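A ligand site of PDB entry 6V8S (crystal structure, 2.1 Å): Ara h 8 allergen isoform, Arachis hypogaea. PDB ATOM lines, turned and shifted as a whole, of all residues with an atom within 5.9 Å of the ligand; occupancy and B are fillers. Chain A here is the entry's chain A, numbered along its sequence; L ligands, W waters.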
ATOM      1  N   ILE A  38     -26.867   9.915 -13.525  1.00  0.00           N
ATOM      2  CA  ILE A  38     -25.399   9.618 -13.503  1.00  0.00           C
ATOM      3  C   ILE A  38     -25.090   8.445 -14.424  1.00  0.00           C
ATOM      4  O   ILE A  38     -25.610   7.367 -14.231  1.00  0.00           O
ATOM      5  CB  ILE A  38     -24.909   9.408 -12.062  1.00  0.00           C
ATOM      6  CG1 ILE A  38     -25.050  10.710 -11.272  1.00  0.00           C
ATOM      7  CG2 ILE A  38     -23.478   8.840 -12.042  1.00  0.00           C
ATOM      8  CD1 ILE A  38     -24.734  10.544  -9.807  1.00  0.00           C
ATOM      9  N   VAL A  56     -17.175  12.168 -12.712  1.00  0.00           N
ATOM     10  CA  VAL A  56     -18.590  11.784 -12.597  1.00  0.00           C
ATOM     11  C   VAL A  56     -19.325  12.462 -13.762  1.00  0.00           C
ATOM     12  O   VAL A  56     -19.400  13.689 -13.785  1.00  0.00           O
ATOM     13  CB  VAL A  56     -19.171  12.188 -11.246  1.00  0.00           C
ATOM     14  CG1 VAL A  56     -20.635  11.746 -11.121  1.00  0.00           C
ATOM     15  CG2 VAL A  56     -18.344  11.638 -10.093  1.00  0.00           C
ATOM     16  N   THR A  57     -19.865  11.648 -14.695  1.00  0.00           N
ATOM     17  CA  THR A  57     -20.598  12.162 -15.852  1.00  0.00           C
ATOM     18  C   THR A  57     -22.093  12.014 -15.613  1.00  0.00           C
ATOM     19  O   THR A  57     -22.494  10.937 -15.193  1.00  0.00           O
ATOM     20  CB  THR A  57     -20.134  11.407 -17.098  1.00  0.00           C
ATOM     21  OG1 THR A  57     -20.402  10.050 -16.846  1.00  0.00           O
ATOM     22  CG2 THR A  57     -18.662  11.669 -17.258  1.00  0.00           C
ATOM     23  N   ALA A  58     -22.886  13.035 -15.933  1.00  0.00           N
ATOM     24  CA  ALA A  58     -24.346  12.975 -15.774  1.00  0.00           C
ATOM     25  C   ALA A  58     -25.038  13.697 -16.930  1.00  0.00           C
ATOM     26  O   ALA A  58     -24.385  14.539 -17.562  1.00  0.00           O
ATOM     27  CB  ALA A  58     -24.761  13.575 -14.488  1.00  0.00           C
ATOM     28  N   VAL A  59     -26.305  13.409 -17.119  1.00  0.00           N
ATOM     29  CA  VAL A  59     -27.130  13.989 -18.217  1.00  0.00           C
ATOM     30  C   VAL A  59     -28.317  14.717 -17.592  1.00  0.00           C
ATOM     31  O   VAL A  59     -28.912  14.176 -16.664  1.00  0.00           O
ATOM     32  CB  VAL A  59     -27.624  12.915 -19.202  1.00  0.00           C
ATOM     33  CG1 VAL A  59     -28.680  13.481 -20.127  1.00  0.00           C
ATOM     34  CG2 VAL A  59     -26.487  12.329 -20.019  1.00  0.00           C
ATOM     35  N   GLU A  60     -28.572  15.947 -18.043  1.00  0.00           N
ATOM     36  CA  GLU A  60     -29.730  16.729 -17.578  1.00  0.00           C
ATOM     37  C   GLU A  60     -30.243  17.579 -18.729  1.00  0.00           C
ATOM     38  O   GLU A  60     -29.466  18.241 -19.356  1.00  0.00           O
ATOM     39  CB  GLU A  60     -29.378  17.611 -16.387  1.00  0.00           C
ATOM     40  CG  GLU A  60     -27.900  17.783 -16.186  1.00  0.00           C
ATOM     41  CD  GLU A  60     -27.565  18.311 -14.815  1.00  0.00           C
ATOM     42  OE1 GLU A  60     -28.485  18.789 -14.146  1.00  0.00           O
ATOM     43  OE2 GLU A  60     -26.408  18.224 -14.455  1.00  0.00           O
ATOM     44  N   SER A  65     -22.677  16.577 -18.938  1.00  0.00           N
ATOM     45  CA  SER A  65     -21.551  17.286 -18.298  1.00  0.00           C
ATOM     46  C   SER A  65     -20.903  16.381 -17.253  1.00  0.00           C
ATOM     47  O   SER A  65     -21.395  15.266 -17.037  1.00  0.00           O
ATOM     48  CB  SER A  65     -21.972  18.613 -17.716  1.00  0.00           C
ATOM     49  OG  SER A  65     -22.977  18.445 -16.773  1.00  0.00           O
ATOM     50  N   TYR A  66     -19.823  16.844 -16.639  1.00  0.00           N
ATOM     51  CA  TYR A  66     -19.112  16.070 -15.596  1.00  0.00           C
ATOM     52  C   TYR A  66     -18.595  16.996 -14.495  1.00  0.00           C
ATOM     53  O   TYR A  66     -18.443  18.220 -14.747  1.00  0.00           O
ATOM     54  CB  TYR A  66     -17.983  15.247 -16.227  1.00  0.00           C
ATOM     55  CG  TYR A  66     -16.858  16.068 -16.785  1.00  0.00           C
ATOM     56  CD1 TYR A  66     -16.847  16.544 -18.066  1.00  0.00           C
ATOM     57  CD2 TYR A  66     -15.746  16.315 -15.977  1.00  0.00           C
ATOM     58  CE1 TYR A  66     -15.786  17.308 -18.545  1.00  0.00           C
ATOM     59  CE2 TYR A  66     -14.674  17.067 -16.440  1.00  0.00           C
ATOM     60  CZ  TYR A  66     -14.689  17.538 -17.733  1.00  0.00           C
ATOM     61  OH  TYR A  66     -13.674  18.354 -18.164  1.00  0.00           O
ATOM     62  N   VAL A  67     -18.276  16.409 -13.346  1.00  0.00           N
ATOM     63  CA  VAL A  67     -17.527  17.070 -12.239  1.00  0.00           C
ATOM     64  C   VAL A  67     -16.417  16.126 -11.801  1.00  0.00           C
ATOM     65  O   VAL A  67     -16.467  14.918 -12.213  1.00  0.00           O
ATOM     66  CB  VAL A  67     -18.432  17.480 -11.062  1.00  0.00           C
ATOM     67  CG1 VAL A  67     -19.599  18.313 -11.539  1.00  0.00           C
ATOM     68  CG2 VAL A  67     -18.959  16.304 -10.296  1.00  0.00           C
ATOM     69  N   ILE A  85     -15.640  17.856  -4.205  1.00  0.00           N
ATOM     70  CA  ILE A  85     -16.222  17.991  -5.568  1.00  0.00           C
ATOM     71  C   ILE A  85     -15.806  19.351  -6.138  1.00  0.00           C
ATOM     72  O   ILE A  85     -15.997  20.419  -5.441  1.00  0.00           O
ATOM     73  CB  ILE A  85     -17.747  17.807  -5.550  1.00  0.00           C
ATOM     74  CG1 ILE A  85     -18.143  16.467  -4.928  1.00  0.00           C
ATOM     75  CG2 ILE A  85     -18.294  17.880  -6.987  1.00  0.00           C
ATOM     76  CD1 ILE A  85     -19.653  16.309  -4.706  1.00  0.00           C
ATOM     77  N   GLY A  90     -19.990  20.582 -15.263  1.00  0.00           N
ATOM     78  CA  GLY A  90     -21.316  20.392 -14.646  1.00  0.00           C
ATOM     79  C   GLY A  90     -21.397  21.069 -13.278  1.00  0.00           C
ATOM     80  O   GLY A  90     -22.449  20.924 -12.627  1.00  0.00           O
ATOM     81  N   PHE A  91     -20.322  21.692 -12.772  1.00  0.00           N
ATOM     82  CA  PHE A  91     -20.280  22.148 -11.345  1.00  0.00           C
ATOM     83  C   PHE A  91     -21.070  23.455 -11.198  1.00  0.00           C
ATOM     84  O   PHE A  91     -21.170  24.229 -12.138  1.00  0.00           O
ATOM     85  CB  PHE A  91     -18.835  22.347 -10.885  1.00  0.00           C
ATOM     86  CG  PHE A  91     -18.651  22.419  -9.395  1.00  0.00           C
ATOM     87  CD1 PHE A  91     -19.249  21.472  -8.578  1.00  0.00           C
ATOM     88  CD2 PHE A  91     -17.913  23.423  -8.775  1.00  0.00           C
ATOM     89  CE1 PHE A  91     -19.119  21.494  -7.211  1.00  0.00           C
ATOM     90  CE2 PHE A  91     -17.698  23.403  -7.405  1.00  0.00           C
ATOM     91  CZ  PHE A  91     -18.333  22.432  -6.637  1.00  0.00           C
ATOM     92  N   GLN A  92     -21.558  23.709  -9.997  1.00  0.00           N
ATOM     93  CA  GLN A  92     -22.234  24.980  -9.615  1.00  0.00           C
ATOM     94  C   GLN A  92     -21.336  26.166 -10.001  1.00  0.00           C
ATOM     95  O   GLN A  92     -20.140  26.180  -9.610  1.00  0.00           O
ATOM     96  CB  GLN A  92     -22.547  25.003  -8.114  1.00  0.00           C
ATOM     97  CG  GLN A  92     -23.126  23.689  -7.549  1.00  0.00           C
ATOM     98  CD  GLN A  92     -24.630  23.588  -7.684  1.00  0.00           C
ATOM     99  OE1 GLN A  92     -25.298  24.587  -7.993  1.00  0.00           O
ATOM    100  NE2 GLN A  92     -25.126  22.368  -7.560  1.00  0.00           N
ATOM    101  N   LEU A  95     -19.425  28.233  -7.194  1.00  0.00           N
ATOM    102  CA  LEU A  95     -18.558  27.442  -6.302  1.00  0.00           C
ATOM    103  C   LEU A  95     -17.185  27.230  -6.953  1.00  0.00           C
ATOM    104  O   LEU A  95     -17.133  26.821  -8.130  1.00  0.00           O
ATOM    105  CB  LEU A  95     -19.204  26.092  -5.996  1.00  0.00           C
ATOM    106  CG  LEU A  95     -20.420  26.126  -5.063  1.00  0.00           C
ATOM    107  CD1 LEU A  95     -20.907  24.759  -4.721  1.00  0.00           C
ATOM    108  CD2 LEU A  95     -20.152  26.920  -3.769  1.00  0.00           C
ATOM    109  N   VAL A  98     -16.592  22.100  -3.170  1.00  0.00           N
ATOM    110  CA  VAL A  98     -17.254  21.715  -1.886  1.00  0.00           C
ATOM    111  C   VAL A  98     -16.509  20.525  -1.319  1.00  0.00           C
ATOM    112  O   VAL A  98     -16.309  19.528  -2.064  1.00  0.00           O
ATOM    113  CB  VAL A  98     -18.767  21.402  -2.073  1.00  0.00           C
ATOM    114  CG1 VAL A  98     -19.482  21.282  -0.740  1.00  0.00           C
ATOM    115  CG2 VAL A  98     -19.401  22.336  -3.002  1.00  0.00           C
ATOM    116  N   PHE A 100     -16.229  17.596   1.664  1.00  0.00           N
ATOM    117  CA  PHE A 100     -17.058  16.737   2.558  1.00  0.00           C
ATOM    118  C   PHE A 100     -16.109  15.938   3.464  1.00  0.00           C
ATOM    119  O   PHE A 100     -15.089  15.384   2.989  1.00  0.00           O
ATOM    120  CB  PHE A 100     -17.898  15.765   1.730  1.00  0.00           C
ATOM    121  CG  PHE A 100     -18.921  16.410   0.842  1.00  0.00           C
ATOM    122  CD1 PHE A 100     -18.596  16.836  -0.424  1.00  0.00           C
ATOM    123  CD2 PHE A 100     -20.228  16.564   1.259  1.00  0.00           C
ATOM    124  CE1 PHE A 100     -19.516  17.442  -1.246  1.00  0.00           C
ATOM    125  CE2 PHE A 100     -21.186  17.106   0.407  1.00  0.00           C
ATOM    126  CZ  PHE A 100     -20.808  17.586  -0.823  1.00  0.00           C
ATOM    127  N   ASP A 134     -29.272  22.385  -3.431  1.00  0.00           N
ATOM    128  CA  ASP A 134     -28.993  21.470  -4.565  1.00  0.00           C
ATOM    129  C   ASP A 134     -27.846  20.508  -4.188  1.00  0.00           C
ATOM    130  O   ASP A 134     -27.993  19.284  -4.425  1.00  0.00           O
ATOM    131  CB  ASP A 134     -28.711  22.247  -5.841  1.00  0.00           C
ATOM    132  CG  ASP A 134     -28.640  21.353  -7.044  1.00  0.00           C
ATOM    133  OD1 ASP A 134     -29.619  20.558  -7.273  1.00  0.00           O
ATOM    134  OD2 ASP A 134     -27.599  21.395  -7.735  1.00  0.00           O
ATOM    135  N   VAL A 135     -26.762  20.999  -3.594  1.00  0.00           N
ATOM    136  CA  VAL A 135     -25.641  20.106  -3.183  1.00  0.00           C
ATOM    137  C   VAL A 135     -26.121  19.123  -2.107  1.00  0.00           C
ATOM    138  O   VAL A 135     -25.735  17.950  -2.154  1.00  0.00           O
ATOM    139  CB  VAL A 135     -24.418  20.943  -2.726  1.00  0.00           C
ATOM    140  CG1 VAL A 135     -23.348  20.071  -2.118  1.00  0.00           C
ATOM    141  CG2 VAL A 135     -23.870  21.746  -3.885  1.00  0.00           C
ATOM    142  N   LYS A 138     -28.551  16.385  -3.640  1.00  0.00           N
ATOM    143  CA  LYS A 138     -27.785  15.411  -4.455  1.00  0.00           C
ATOM    144  C   LYS A 138     -26.963  14.498  -3.553  1.00  0.00           C
ATOM    145  O   LYS A 138     -26.902  13.269  -3.852  1.00  0.00           O
ATOM    146  CB  LYS A 138     -26.873  16.113  -5.458  1.00  0.00           C
ATOM    147  CG  LYS A 138     -27.634  16.804  -6.569  1.00  0.00           C
ATOM    148  CD  LYS A 138     -26.754  17.650  -7.451  1.00  0.00           C
ATOM    149  CE  LYS A 138     -27.509  18.071  -8.697  1.00  0.00           C
ATOM    150  NZ  LYS A 138     -26.875  19.196  -9.363  1.00  0.00           N
ATOM    151  N   SER A 139     -26.349  15.057  -2.507  1.00  0.00           N
ATOM    152  CA  SER A 139     -25.493  14.295  -1.564  1.00  0.00           C
ATOM    153  C   SER A 139     -26.385  13.296  -0.843  1.00  0.00           C
ATOM    154  O   SER A 139     -25.984  12.119  -0.709  1.00  0.00           O
ATOM    155  CB  SER A 139     -24.810  15.214  -0.555  1.00  0.00           C
ATOM    156  OG  SER A 139     -23.881  16.032  -1.286  1.00  0.00           O
ATOM    157  N   ILE A 142     -27.818  10.380  -3.343  1.00  0.00           N
ATOM    158  CA  ILE A 142     -26.871   9.278  -3.645  1.00  0.00           C
ATOM    159  C   ILE A 142     -26.770   8.357  -2.436  1.00  0.00           C
ATOM    160  O   ILE A 142     -26.947   7.118  -2.599  1.00  0.00           O
ATOM    161  CB  ILE A 142     -25.517   9.854  -4.055  1.00  0.00           C
ATOM    162  CG1 ILE A 142     -25.640  10.418  -5.459  1.00  0.00           C
ATOM    163  CG2 ILE A 142     -24.410   8.804  -3.905  1.00  0.00           C
ATOM    164  CD1 ILE A 142     -24.472  11.319  -5.810  1.00  0.00           C
HETATM  165  C1  LIG L   1     -22.928  15.968  -8.827  1.00  0.00           C
HETATM  166  C2  LIG L   1     -22.893  14.649  -9.140  1.00  0.00           C
HETATM  167  C3  LIG L   1     -22.781  13.656  -8.156  1.00  0.00           C
HETATM  168  C4  LIG L   1     -22.790  13.998  -6.853  1.00  0.00           C
HETATM  169  C5  LIG L   1     -22.827  15.357  -6.464  1.00  0.00           C
HETATM  170  C6  LIG L   1     -22.793  15.673  -5.087  1.00  0.00           C
HETATM  171  C7  LIG L   1     -22.805  16.943  -4.667  1.00  0.00           C
HETATM  172  C8  LIG L   1     -22.826  17.988  -5.610  1.00  0.00           C
HETATM  173  N1  LIG L   1     -23.068  16.911  -9.868  1.00  0.00           N
HETATM  174  S1  LIG L   1     -22.900  19.185  -7.969  1.00  0.00           S
HETATM  175  C9  LIG L   1     -22.928  17.742  -6.949  1.00  0.00           C
HETATM  176  C10 LIG L   1     -22.891  16.393  -7.447  1.00  0.00           C
HETATM  177  C11 LIG L   1     -22.967  16.709 -11.259  1.00  0.00           C
HETATM  178  C12 LIG L   1     -23.656  17.588 -12.093  1.00  0.00           C
HETATM  179  C13 LIG L   1     -23.571  17.455 -13.478  1.00  0.00           C
HETATM  180  C14 LIG L   1     -22.792  16.479 -14.036  1.00  0.00           C
HETATM  181  C15 LIG L   1     -22.097  15.615 -13.220  1.00  0.00           C
HETATM  182  C16 LIG L   1     -22.169  15.728 -11.841  1.00  0.00           C
HETATM  183  O1  LIG L   1     -24.179  19.143  -8.887  1.00  0.00           O
HETATM  184  O2  LIG L   1     -23.037  20.332  -7.126  1.00  0.00           O
HETATM  185  O3  LIG L   1     -21.700  19.104  -8.757  1.00  0.00           O
HETATM  186  O   HOH W   1     -23.943  21.346 -10.649  1.00  0.00           O
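NZ of Lys 138 lies within salt-bridge range of O1 of the ligand (2.7 Å). NE2 of Gln 92 lies within hydrogen-bond range of O2 of the ligand, at 2.9 Å.
The side-chain amino group of Lys 138 lies within salt-bridge range of the side-chain carboxylate of Asp 134 (2.8 Å). The side-chain carboxylate of Asp 134 sits at hydrogen-bond distance from the side-chain amide nitrogen of Gln 92, 2.7 Å away. N of Ile 85 is in hydrogen-bond range of O of Val 98. The backbone NH (N) of Val 56 lies within hydrogen-bond range of the backbone carbonyl oxygen (O) of Val 67, 2.9 Å away. The backbone carbonyl oxygen of Ser 65 sits at hydrogen-bond distance from the backbone NH of Ala 58 (2.9 Å). The backbone carbonyl oxygen of Tyr 66 sits at hydrogen-bond distance from the backbone NH of Gly 90 (2.9 Å). O of Val 135 sits at hydrogen-bond distance from OG of Ser 139.
Merely in contact with the ligand: Glu 60 (3.1 Å), Ile 85 (3.2 Å), Ile 142 (3.3 Å), Val 56 (3.4 Å), Ser 65 (3.4 Å), Phe 91 (3.4 Å), Ala 58 (3.5 Å), Val 67 (3.6 Å), Gly 90 (3.6 Å), Val 135 (3.6 Å), Ser 139 (3.7 Å) and Tyr 66 (3.8 Å). Hydrophobic or aromatic side chains within 4 Å of the ligand: Ala 58, Val 67, Ile 85, Phe 91, Val 135 and Ile 142.
Water W1 lies within hydrogen-bond range of the backbone carbonyl oxygen of Gly 90 (2.5 Å), an oxygen (O1) of the ligand (2.8 Å) and the backbone NH of Gln 92 (3.4 Å).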
